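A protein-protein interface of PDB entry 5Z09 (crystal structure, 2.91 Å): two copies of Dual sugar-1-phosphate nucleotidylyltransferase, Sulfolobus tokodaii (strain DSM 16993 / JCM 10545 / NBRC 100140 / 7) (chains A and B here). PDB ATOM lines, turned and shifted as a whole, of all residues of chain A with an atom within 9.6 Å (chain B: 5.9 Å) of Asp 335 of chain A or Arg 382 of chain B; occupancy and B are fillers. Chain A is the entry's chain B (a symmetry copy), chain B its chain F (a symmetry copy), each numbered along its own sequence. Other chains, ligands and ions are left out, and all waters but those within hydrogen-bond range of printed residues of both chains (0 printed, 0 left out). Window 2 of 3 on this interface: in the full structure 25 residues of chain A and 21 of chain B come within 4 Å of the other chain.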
ATOM      1  N   LEU A 332     -19.803  22.336 -12.839  1.00  0.00           N
ATOM      2  CA  LEU A 332     -21.202  22.422 -12.459  1.00  0.00           C
ATOM      3  C   LEU A 332     -21.456  21.407 -11.377  1.00  0.00           C
ATOM      4  O   LEU A 332     -21.003  20.281 -11.476  1.00  0.00           O
ATOM      5  CB  LEU A 332     -22.123  22.132 -13.655  1.00  0.00           C
ATOM      6  CG  LEU A 332     -23.612  22.419 -13.448  1.00  0.00           C
ATOM      7  CD1 LEU A 332     -23.881  23.919 -13.517  1.00  0.00           C
ATOM      8  CD2 LEU A 332     -24.460  21.684 -14.471  1.00  0.00           C
ATOM      9  N   ARG A 333     -22.223  21.799 -10.365  1.00  0.00           N
ATOM     10  CA  ARG A 333     -22.664  20.884  -9.317  1.00  0.00           C
ATOM     11  C   ARG A 333     -23.955  20.199  -9.709  1.00  0.00           C
ATOM     12  O   ARG A 333     -24.666  20.674 -10.605  1.00  0.00           O
ATOM     13  CB  ARG A 333     -22.866  21.666  -8.034  1.00  0.00           C
ATOM     14  CG  ARG A 333     -21.560  21.957  -7.311  1.00  0.00           C
ATOM     15  CD  ARG A 333     -21.738  22.823  -6.084  1.00  0.00           C
ATOM     16  NE  ARG A 333     -22.871  22.385  -5.273  1.00  0.00           N
ATOM     17  CZ  ARG A 333     -23.208  22.930  -4.114  1.00  0.00           C
ATOM     18  NH1 ARG A 333     -22.510  23.946  -3.631  1.00  0.00           N
ATOM     19  NH2 ARG A 333     -24.251  22.467  -3.445  1.00  0.00           N
ATOM     20  N   PHE A 334     -24.195  19.016  -9.147  1.00  0.00           N
ATOM     21  CA  PHE A 334     -25.336  18.194  -9.590  1.00  0.00           C
ATOM     22  C   PHE A 334     -26.658  18.921  -9.364  1.00  0.00           C
ATOM     23  O   PHE A 334     -27.487  19.000 -10.267  1.00  0.00           O
ATOM     24  CB  PHE A 334     -25.346  16.836  -8.895  1.00  0.00           C
ATOM     25  CG  PHE A 334     -24.501  15.802  -9.573  1.00  0.00           C
ATOM     26  CD1 PHE A 334     -23.580  15.063  -8.850  1.00  0.00           C
ATOM     27  CD2 PHE A 334     -24.628  15.557 -10.931  1.00  0.00           C
ATOM     28  CE1 PHE A 334     -22.806  14.095  -9.469  1.00  0.00           C
ATOM     29  CE2 PHE A 334     -23.836  14.611 -11.560  1.00  0.00           C
ATOM     30  CZ  PHE A 334     -22.931  13.872 -10.825  1.00  0.00           C
ATOM     31  N   ASP A 335     -26.763  19.574  -8.209  1.00  0.00           N
ATOM     32  CA  ASP A 335     -27.943  20.369  -7.836  1.00  0.00           C
ATOM     33  C   ASP A 335     -28.041  21.764  -8.494  1.00  0.00           C
ATOM     34  O   ASP A 335     -29.014  22.494  -8.273  1.00  0.00           O
ATOM     35  CB  ASP A 335     -27.971  20.517  -6.307  1.00  0.00           C
ATOM     36  CG  ASP A 335     -26.718  21.170  -5.755  1.00  0.00           C
ATOM     37  OD1 ASP A 335     -26.189  22.108  -6.392  1.00  0.00           O
ATOM     38  OD2 ASP A 335     -26.230  20.707  -4.704  1.00  0.00           O
ATOM     39  N   GLU A 336     -26.984  22.172  -9.192  1.00  0.00           N
ATOM     40  CA  GLU A 336     -26.933  23.452  -9.897  1.00  0.00           C
ATOM     41  C   GLU A 336     -26.980  24.665  -8.965  1.00  0.00           C
ATOM     42  O   GLU A 336     -27.115  25.809  -9.431  1.00  0.00           O
ATOM     43  CB  GLU A 336     -28.049  23.547 -10.934  1.00  0.00           C
ATOM     44  CG  GLU A 336     -28.064  22.381 -11.910  1.00  0.00           C
ATOM     45  CD  GLU A 336     -28.526  22.778 -13.296  1.00  0.00           C
ATOM     46  OE1 GLU A 336     -28.524  23.989 -13.608  1.00  0.00           O
ATOM     47  OE2 GLU A 336     -28.818  21.869 -14.103  1.00  0.00           O
ATOM     48  N   LYS A 337     -26.727  24.434  -7.675  1.00  0.00           N
ATOM     49  CA  LYS A 337     -26.453  25.525  -6.744  1.00  0.00           C
ATOM     50  C   LYS A 337     -25.092  26.128  -7.035  1.00  0.00           C
ATOM     51  O   LYS A 337     -24.259  25.530  -7.720  1.00  0.00           O
ATOM     52  CB  LYS A 337     -26.501  25.059  -5.283  1.00  0.00           C
ATOM     53  CG  LYS A 337     -27.854  25.241  -4.604  1.00  0.00           C
ATOM     54  CD  LYS A 337     -28.647  23.942  -4.555  1.00  0.00           C
ATOM     55  CE  LYS A 337     -30.149  24.171  -4.673  1.00  0.00           C
ATOM     56  NZ  LYS A 337     -30.831  24.168  -3.348  1.00  0.00           N
ATOM     57  N   GLU A 338     -24.887  27.329  -6.518  1.00  0.00           N
ATOM     58  CA  GLU A 338     -23.659  28.075  -6.745  1.00  0.00           C
ATOM     59  C   GLU A 338     -22.491  27.329  -6.136  1.00  0.00           C
ATOM     60  O   GLU A 338     -22.638  26.646  -5.126  1.00  0.00           O
ATOM     61  CB  GLU A 338     -23.765  29.475  -6.137  1.00  0.00           C
ATOM     62  CG  GLU A 338     -24.886  30.324  -6.741  1.00  0.00           C
ATOM     63  CD  GLU A 338     -24.951  31.727  -6.171  1.00  0.00           C
ATOM     64  OE1 GLU A 338     -24.486  31.927  -5.031  1.00  0.00           O
ATOM     65  OE2 GLU A 338     -25.458  32.628  -6.869  1.00  0.00           O
ATOM     66  N   VAL A 339     -21.376  27.326  -6.856  1.00  0.00           N
ATOM     67  CA  VAL A 339     -20.221  26.564  -6.458  1.00  0.00           C
ATOM     68  C   VAL A 339     -19.553  27.299  -5.306  1.00  0.00           C
ATOM     69  O   VAL A 339     -19.421  28.525  -5.342  1.00  0.00           O
ATOM     70  CB  VAL A 339     -19.230  26.414  -7.626  1.00  0.00           C
ATOM     71  CG1 VAL A 339     -17.944  25.705  -7.181  1.00  0.00           C
ATOM     72  CG2 VAL A 339     -19.888  25.665  -8.765  1.00  0.00           C
ATOM     73  N   LYS A 340     -19.118  26.545  -4.298  1.00  0.00           N
ATOM     74  CA  LYS A 340     -18.490  27.135  -3.127  1.00  0.00           C
ATOM     75  C   LYS A 340     -16.988  26.871  -3.132  1.00  0.00           C
ATOM     76  O   LYS A 340     -16.508  25.934  -3.761  1.00  0.00           O
ATOM     77  CB  LYS A 340     -19.135  26.614  -1.837  1.00  0.00           C
ATOM     78  CG  LYS A 340     -20.654  26.621  -1.910  1.00  0.00           C
ATOM     79  CD  LYS A 340     -21.324  26.874  -0.573  1.00  0.00           C
ATOM     80  CE  LYS A 340     -22.799  27.172  -0.775  1.00  0.00           C
ATOM     81  NZ  LYS A 340     -23.600  26.855   0.438  1.00  0.00           N
ATOM     82  N   ARG A 347     -15.705  28.536   3.980  1.00  0.00           N
ATOM     83  CA  ARG A 347     -16.430  28.015   2.824  1.00  0.00           C
ATOM     84  C   ARG A 347     -17.504  29.024   2.393  1.00  0.00           C
ATOM     85  O   ARG A 347     -18.407  29.346   3.154  1.00  0.00           O
ATOM     86  CB  ARG A 347     -17.078  26.685   3.209  1.00  0.00           C
ATOM     87  CG  ARG A 347     -17.775  25.950   2.082  1.00  0.00           C
ATOM     88  CD  ARG A 347     -16.842  24.953   1.432  1.00  0.00           C
ATOM     89  NE  ARG A 347     -17.559  23.988   0.614  1.00  0.00           N
ATOM     90  CZ  ARG A 347     -17.050  23.404  -0.467  1.00  0.00           C
ATOM     91  NH1 ARG A 347     -15.809  23.676  -0.869  1.00  0.00           N
ATOM     92  NH2 ARG A 347     -17.795  22.555  -1.164  1.00  0.00           N
ATOM     93  N   ARG A 352     -21.342  31.959  -8.537  1.00  0.00           N
ATOM     94  CA  ARG A 352     -21.340  31.400  -9.881  1.00  0.00           C
ATOM     95  C   ARG A 352     -22.046  30.051  -9.848  1.00  0.00           C
ATOM     96  O   ARG A 352     -21.687  29.188  -9.065  1.00  0.00           O
ATOM     97  CB  ARG A 352     -19.903  31.234 -10.395  1.00  0.00           C
ATOM     98  CG  ARG A 352     -19.234  32.536 -10.830  1.00  0.00           C
ATOM     99  CD  ARG A 352     -17.801  32.295 -11.298  1.00  0.00           C
ATOM    100  NE  ARG A 352     -17.708  31.677 -12.634  1.00  0.00           N
ATOM    101  CZ  ARG A 352     -17.478  32.337 -13.777  1.00  0.00           C
ATOM    102  NH1 ARG A 352     -17.330  33.656 -13.798  1.00  0.00           N
ATOM    103  NH2 ARG A 352     -17.364  31.680 -14.920  1.00  0.00           N
ATOM    104  N   ARG A 353     -23.002  29.851 -10.747  1.00  0.00           N
ATOM    105  CA  ARG A 353     -23.567  28.526 -10.990  1.00  0.00           C
ATOM    106  C   ARG A 353     -22.546  27.568 -11.637  1.00  0.00           C
ATOM    107  O   ARG A 353     -22.525  26.357 -11.343  1.00  0.00           O
ATOM    108  CB  ARG A 353     -24.799  28.642 -11.883  1.00  0.00           C
ATOM    109  CG  ARG A 353     -25.351  27.309 -12.358  1.00  0.00           C
ATOM    110  CD  ARG A 353     -26.753  27.439 -12.915  1.00  0.00           C
ATOM    111  NE  ARG A 353     -27.013  26.396 -13.904  1.00  0.00           N
ATOM    112  CZ  ARG A 353     -26.645  26.461 -15.181  1.00  0.00           C
ATOM    113  NH1 ARG A 353     -25.969  27.509 -15.650  1.00  0.00           N
ATOM    114  NH2 ARG A 353     -26.968  25.471 -16.003  1.00  0.00           N
ATOM    115  N   PRO A 373     -15.577  20.867  -8.846  1.00  0.00           N
ATOM    116  CA  PRO A 373     -15.841  22.295  -8.933  1.00  0.00           C
ATOM    117  C   PRO A 373     -15.357  22.994  -7.693  1.00  0.00           C
ATOM    118  O   PRO A 373     -15.386  22.415  -6.612  1.00  0.00           O
ATOM    119  CB  PRO A 373     -17.361  22.359  -9.017  1.00  0.00           C
ATOM    120  CG  PRO A 373     -17.773  21.053  -9.608  1.00  0.00           C
ATOM    121  CD  PRO A 373     -16.816  20.077  -8.994  1.00  0.00           C
ATOM    122  N   VAL B 363     -31.244  11.934 -16.232  1.00  0.00           N
ATOM    123  CA  VAL B 363     -29.969  11.511 -15.648  1.00  0.00           C
ATOM    124  C   VAL B 363     -28.881  12.561 -15.885  1.00  0.00           C
ATOM    125  O   VAL B 363     -28.822  13.193 -16.950  1.00  0.00           O
ATOM    126  CB  VAL B 363     -29.503  10.182 -16.246  1.00  0.00           C
ATOM    127  CG1 VAL B 363     -28.058   9.908 -15.869  1.00  0.00           C
ATOM    128  CG2 VAL B 363     -30.402   9.045 -15.783  1.00  0.00           C
ATOM    129  N   ARG B 364     -28.054  12.791 -14.872  1.00  0.00           N
ATOM    130  CA  ARG B 364     -26.805  13.515 -15.082  1.00  0.00           C
ATOM    131  C   ARG B 364     -25.617  12.650 -14.687  1.00  0.00           C
ATOM    132  O   ARG B 364     -25.627  12.032 -13.622  1.00  0.00           O
ATOM    133  CB  ARG B 364     -26.782  14.843 -14.323  1.00  0.00           C
ATOM    134  CG  ARG B 364     -25.858  15.865 -14.978  1.00  0.00           C
ATOM    135  CD  ARG B 364     -25.588  17.085 -14.109  1.00  0.00           C
ATOM    136  NE  ARG B 364     -26.784  17.871 -13.811  1.00  0.00           N
ATOM    137  CZ  ARG B 364     -27.262  18.849 -14.578  1.00  0.00           C
ATOM    138  NH1 ARG B 364     -26.679  19.157 -15.736  1.00  0.00           N
ATOM    139  NH2 ARG B 364     -28.348  19.512 -14.190  1.00  0.00           N
ATOM    140  N   THR B 365     -24.643  12.520 -15.587  1.00  0.00           N
ATOM    141  CA  THR B 365     -23.359  11.922 -15.230  1.00  0.00           C
ATOM    142  C   THR B 365     -22.321  13.015 -14.981  1.00  0.00           C
ATOM    143  O   THR B 365     -22.281  14.034 -15.682  1.00  0.00           O
ATOM    144  CB  THR B 365     -22.837  10.978 -16.322  1.00  0.00           C
ATOM    145  OG1 THR B 365     -22.498  11.724 -17.501  1.00  0.00           O
ATOM    146  CG2 THR B 365     -23.875   9.934 -16.672  1.00  0.00           C
ATOM    147  N   TYR B 380     -33.465  10.142 -13.432  1.00  0.00           N
ATOM    148  CA  TYR B 380     -33.220  11.088 -12.340  1.00  0.00           C
ATOM    149  C   TYR B 380     -32.012  10.708 -11.493  1.00  0.00           C
ATOM    150  O   TYR B 380     -31.657  11.432 -10.565  1.00  0.00           O
ATOM    151  CB  TYR B 380     -34.478  11.302 -11.464  1.00  0.00           C
ATOM    152  CG  TYR B 380     -35.545  12.152 -12.139  1.00  0.00           C
ATOM    153  CD1 TYR B 380     -35.321  13.502 -12.398  1.00  0.00           C
ATOM    154  CD2 TYR B 380     -36.737  11.586 -12.601  1.00  0.00           C
ATOM    155  CE1 TYR B 380     -36.249  14.267 -13.089  1.00  0.00           C
ATOM    156  CE2 TYR B 380     -37.654  12.332 -13.327  1.00  0.00           C
ATOM    157  CZ  TYR B 380     -37.427  13.679 -13.537  1.00  0.00           C
ATOM    158  OH  TYR B 380     -38.369  14.458 -14.170  1.00  0.00           O
ATOM    159  N   ALA B 381     -31.320   9.638 -11.876  1.00  0.00           N
ATOM    160  CA  ALA B 381     -30.067   9.265 -11.220  1.00  0.00           C
ATOM    161  C   ALA B 381     -28.986  10.335 -11.410  1.00  0.00           C
ATOM    162  O   ALA B 381     -29.033  11.129 -12.354  1.00  0.00           O
ATOM    163  CB  ALA B 381     -29.578   7.934 -11.749  1.00  0.00           C
ATOM    164  N   ARG B 382     -28.036  10.360 -10.485  1.00  0.00           N
ATOM    165  CA  ARG B 382     -26.825  11.155 -10.628  1.00  0.00           C
ATOM    166  C   ARG B 382     -25.648  10.227 -10.432  1.00  0.00           C
ATOM    167  O   ARG B 382     -25.602   9.491  -9.447  1.00  0.00           O
ATOM    168  CB  ARG B 382     -26.761  12.252  -9.570  1.00  0.00           C
ATOM    169  CG  ARG B 382     -28.002  13.024  -9.356  1.00  0.00           C
ATOM    170  CD  ARG B 382     -27.880  13.912  -8.137  1.00  0.00           C
ATOM    171  NE  ARG B 382     -28.764  15.080  -8.234  1.00  0.00           N
ATOM    172  CZ  ARG B 382     -28.832  16.016  -7.299  1.00  0.00           C
ATOM    173  NH1 ARG B 382     -28.094  15.898  -6.204  1.00  0.00           N
ATOM    174  NH2 ARG B 382     -29.612  17.076  -7.465  1.00  0.00           N
ATOM    175  N   ILE B 383     -24.697  10.252 -11.367  1.00  0.00           N
ATOM    176  CA  ILE B 383     -23.471   9.450 -11.255  1.00  0.00           C
ATOM    177  C   ILE B 383     -22.281  10.328 -10.877  1.00  0.00           C
ATOM    178  O   ILE B 383     -21.939  11.263 -11.601  1.00  0.00           O
ATOM    179  CB  ILE B 383     -23.129   8.739 -12.572  1.00  0.00           C
ATOM    180  CG1 ILE B 383     -24.375   8.136 -13.217  1.00  0.00           C
ATOM    181  CG2 ILE B 383     -22.082   7.671 -12.312  1.00  0.00           C
ATOM    182  CD1 ILE B 383     -25.025   7.029 -12.412  1.00  0.00           C
ATOM    183  N   TYR B 384     -21.695  10.070  -9.711  1.00  0.00           N
ATOM    184  CA  TYR B 384     -20.666  10.961  -9.192  1.00  0.00           C
ATOM    185  C   TYR B 384     -19.355  10.847 -10.030  1.00  0.00           C
ATOM    186  O   TYR B 384     -19.125   9.835 -10.744  1.00  0.00           O
ATOM    187  CB  TYR B 384     -20.584  10.943  -7.661  1.00  0.00           C
ATOM    188  CG  TYR B 384     -21.668  11.816  -7.043  1.00  0.00           C
ATOM    189  CD1 TYR B 384     -23.018  11.557  -7.305  1.00  0.00           C
ATOM    190  CD2 TYR B 384     -21.363  12.872  -6.185  1.00  0.00           C
ATOM    191  CE1 TYR B 384     -24.024  12.312  -6.738  1.00  0.00           C
ATOM    192  CE2 TYR B 384     -22.375  13.642  -5.618  1.00  0.00           C
ATOM    193  CZ  TYR B 384     -23.702  13.352  -5.895  1.00  0.00           C
ATOM    194  OH  TYR B 384     -24.713  14.104  -5.329  1.00  0.00           O
ATOM    195  N   VAL B 393     -28.734   0.985 -11.928  1.00  0.00           N
ATOM    196  CA  VAL B 393     -28.817   2.097 -11.003  1.00  0.00           C
ATOM    197  C   VAL B 393     -30.272   2.520 -10.868  1.00  0.00           C
ATOM    198  O   VAL B 393     -30.995   2.629 -11.862  1.00  0.00           O
ATOM    199  CB  VAL B 393     -27.963   3.278 -11.498  1.00  0.00           C
ATOM    200  CG1 VAL B 393     -28.189   4.514 -10.640  1.00  0.00           C
ATOM    201  CG2 VAL B 393     -26.491   2.893 -11.498  1.00  0.00           C
ATOM    202  N   GLY B 396     -33.639   7.762  -9.337  1.00  0.00           N
ATOM    203  CA  GLY B 396     -33.288   8.766  -8.336  1.00  0.00           C
ATOM    204  C   GLY B 396     -32.003   8.499  -7.558  1.00  0.00           C
ATOM    205  O   GLY B 396     -31.584   9.336  -6.760  1.00  0.00           O
ATOM    206  N   GLU B 397     -31.305   7.410  -7.882  1.00  0.00           N
ATOM    207  CA  GLU B 397     -30.131   7.004  -7.106  1.00  0.00           C
ATOM    208  C   GLU B 397     -28.947   7.952  -7.277  1.00  0.00           C
ATOM    209  O   GLU B 397     -28.640   8.391  -8.385  1.00  0.00           O
ATOM    210  CB  GLU B 397     -29.678   5.602  -7.483  1.00  0.00           C
ATOM    211  CG  GLU B 397     -29.136   4.859  -6.285  1.00  0.00           C
ATOM    212  CD  GLU B 397     -28.179   3.746  -6.643  1.00  0.00           C
ATOM    213  OE1 GLU B 397     -28.581   2.814  -7.374  1.00  0.00           O
ATOM    214  OE2 GLU B 397     -27.042   3.768  -6.122  1.00  0.00           O
ATOM    215  N   PHE B 398     -28.287   8.270  -6.170  1.00  0.00           N
ATOM    216  CA  PHE B 398     -27.030   9.006  -6.209  1.00  0.00           C
ATOM    217  C   PHE B 398     -25.935   7.985  -6.081  1.00  0.00           C
ATOM    218  O   PHE B 398     -25.638   7.524  -4.984  1.00  0.00           O
ATOM    219  CB  PHE B 398     -26.942  10.024  -5.068  1.00  0.00           C
ATOM    220  CG  PHE B 398     -27.974  11.117  -5.143  1.00  0.00           C
ATOM    221  CD1 PHE B 398     -27.934  12.177  -4.252  1.00  0.00           C
ATOM    222  CD2 PHE B 398     -28.971  11.109  -6.125  1.00  0.00           C
ATOM    223  CE1 PHE B 398     -28.849  13.213  -4.347  1.00  0.00           C
ATOM    224  CE2 PHE B 398     -29.887  12.134  -6.217  1.00  0.00           C
ATOM    225  CZ  PHE B 398     -29.817  13.201  -5.339  1.00  0.00           C
ATOM    226  N   PHE B 399     -25.453   7.527  -7.233  1.00  0.00           N
ATOM    227  CA  PHE B 399     -24.452   6.462  -7.316  1.00  0.00           C
ATOM    228  C   PHE B 399     -23.074   7.103  -7.257  1.00  0.00           C
ATOM    229  O   PHE B 399     -22.707   7.829  -8.177  1.00  0.00           O
ATOM    230  CB  PHE B 399     -24.631   5.726  -8.643  1.00  0.00           C
ATOM    231  CG  PHE B 399     -23.682   4.591  -8.838  1.00  0.00           C
ATOM    232  CD1 PHE B 399     -24.091   3.285  -8.614  1.00  0.00           C
ATOM    233  CD2 PHE B 399     -22.396   4.818  -9.297  1.00  0.00           C
ATOM    234  CE1 PHE B 399     -23.226   2.226  -8.818  1.00  0.00           C
ATOM    235  CE2 PHE B 399     -21.525   3.766  -9.504  1.00  0.00           C
ATOM    236  CZ  PHE B 399     -21.942   2.465  -9.264  1.00  0.00           C
ATOM    237  N   LYS B 400     -22.356   6.925  -6.144  1.00  0.00           N
ATOM    238  CA  LYS B 400     -21.125   7.682  -5.937  1.00  0.00           C
ATOM    239  C   LYS B 400     -19.853   6.850  -5.740  1.00  0.00           C
ATOM    240  O   LYS B 400     -18.756   7.411  -5.641  1.00  0.00           O
ATOM    241  CB  LYS B 400     -21.295   8.732  -4.832  1.00  0.00           C
ATOM    242  CG  LYS B 400     -21.793   8.212  -3.501  1.00  0.00           C
ATOM    243  CD  LYS B 400     -20.639   8.019  -2.527  1.00  0.00           C
ATOM    244  CE  LYS B 400     -21.022   7.119  -1.360  1.00  0.00           C
ATOM    245  NZ  LYS B 400     -19.901   6.220  -0.967  1.00  0.00           N
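The guanidinium group (NH2) of Arg 364 of chain B lies within salt-bridge range of the side-chain carboxylate (OE2) of Glu 336 of chain A, 2.4 Å away.
O of Phe 399 of chain B lies within hydrogen-bond range of N of Tyr 384 of chain B (2.9 Å).
The backbone NH (N) of Lys 337 of chain A is in hydrogen-bond range of the side-chain carboxylate (OD1) of Asp 335 of chain A (2.7 Å).
The backbone NH (N) of Arg 382 of chain B sits at hydrogen-bond distance from the backbone carbonyl oxygen (O) of Glu 397 of chain B, 2.9 Å away.
O of Arg 382 of chain B sits at hydrogen-bond distance from N of Phe 399 of chain B.
NH2 of Arg 333 of chain A lies within salt-bridge range of OD2 of Asp 335 of chain A (2.9 Å).
N of Arg 364 of chain B is in hydrogen-bond range of O of Ala 381 of chain B, 3.2 Å away.
Among the printed residues, merely in contact across the chains: Leu 332 of chain A with Arg 364 of chain B, Phe 334 of chain A with Arg 364 of chain B, Phe 334 of chain A with Arg 382 of chain B, Phe 334 of chain A with Ile 383 of chain B, Phe 334 of chain A with Tyr 384 of chain B and Asp 335 of chain A with Arg 382 of chain B.
No residue of chain A comes within 4 Å of Ala 381 of chain B.
Ile 383 of chain B touches one residue of chain A.
Of the printed residues of chain B, Leu 332 of chain A touches Arg 364 (3.6 Å).
Of the printed residues of chain A, Arg 364 of chain B touches Leu 332, Phe 334 and Glu 336.
Lys 340 of chain A touches none of the printed residues of chain B.
The nearest printed residue of chain B that does not touch Asp 335 of chain A is Arg 364 of chain B (5.9 Å).
The nearest printed residue of chain A that does not touch Tyr 384 of chain B is Asp 335 of chain A (6.5 Å).
Printed residues of chain B that touch a printed residue of chain A: Arg 364, Arg 382, Ile 383 and Tyr 384.
Hydrophobic or aromatic side chains of chain B that line the printed part of chain A: Tyr 384.
Of the 13 printed residues of chain A, 4 touch a printed residue of chain B.
Printed residues of chain A that touch a printed residue of chain B: Leu 332, Phe 334, Asp 335 and Glu 336.
Among the printed residues, 7 pairs touch across the chains.
No position is printed for both chains.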
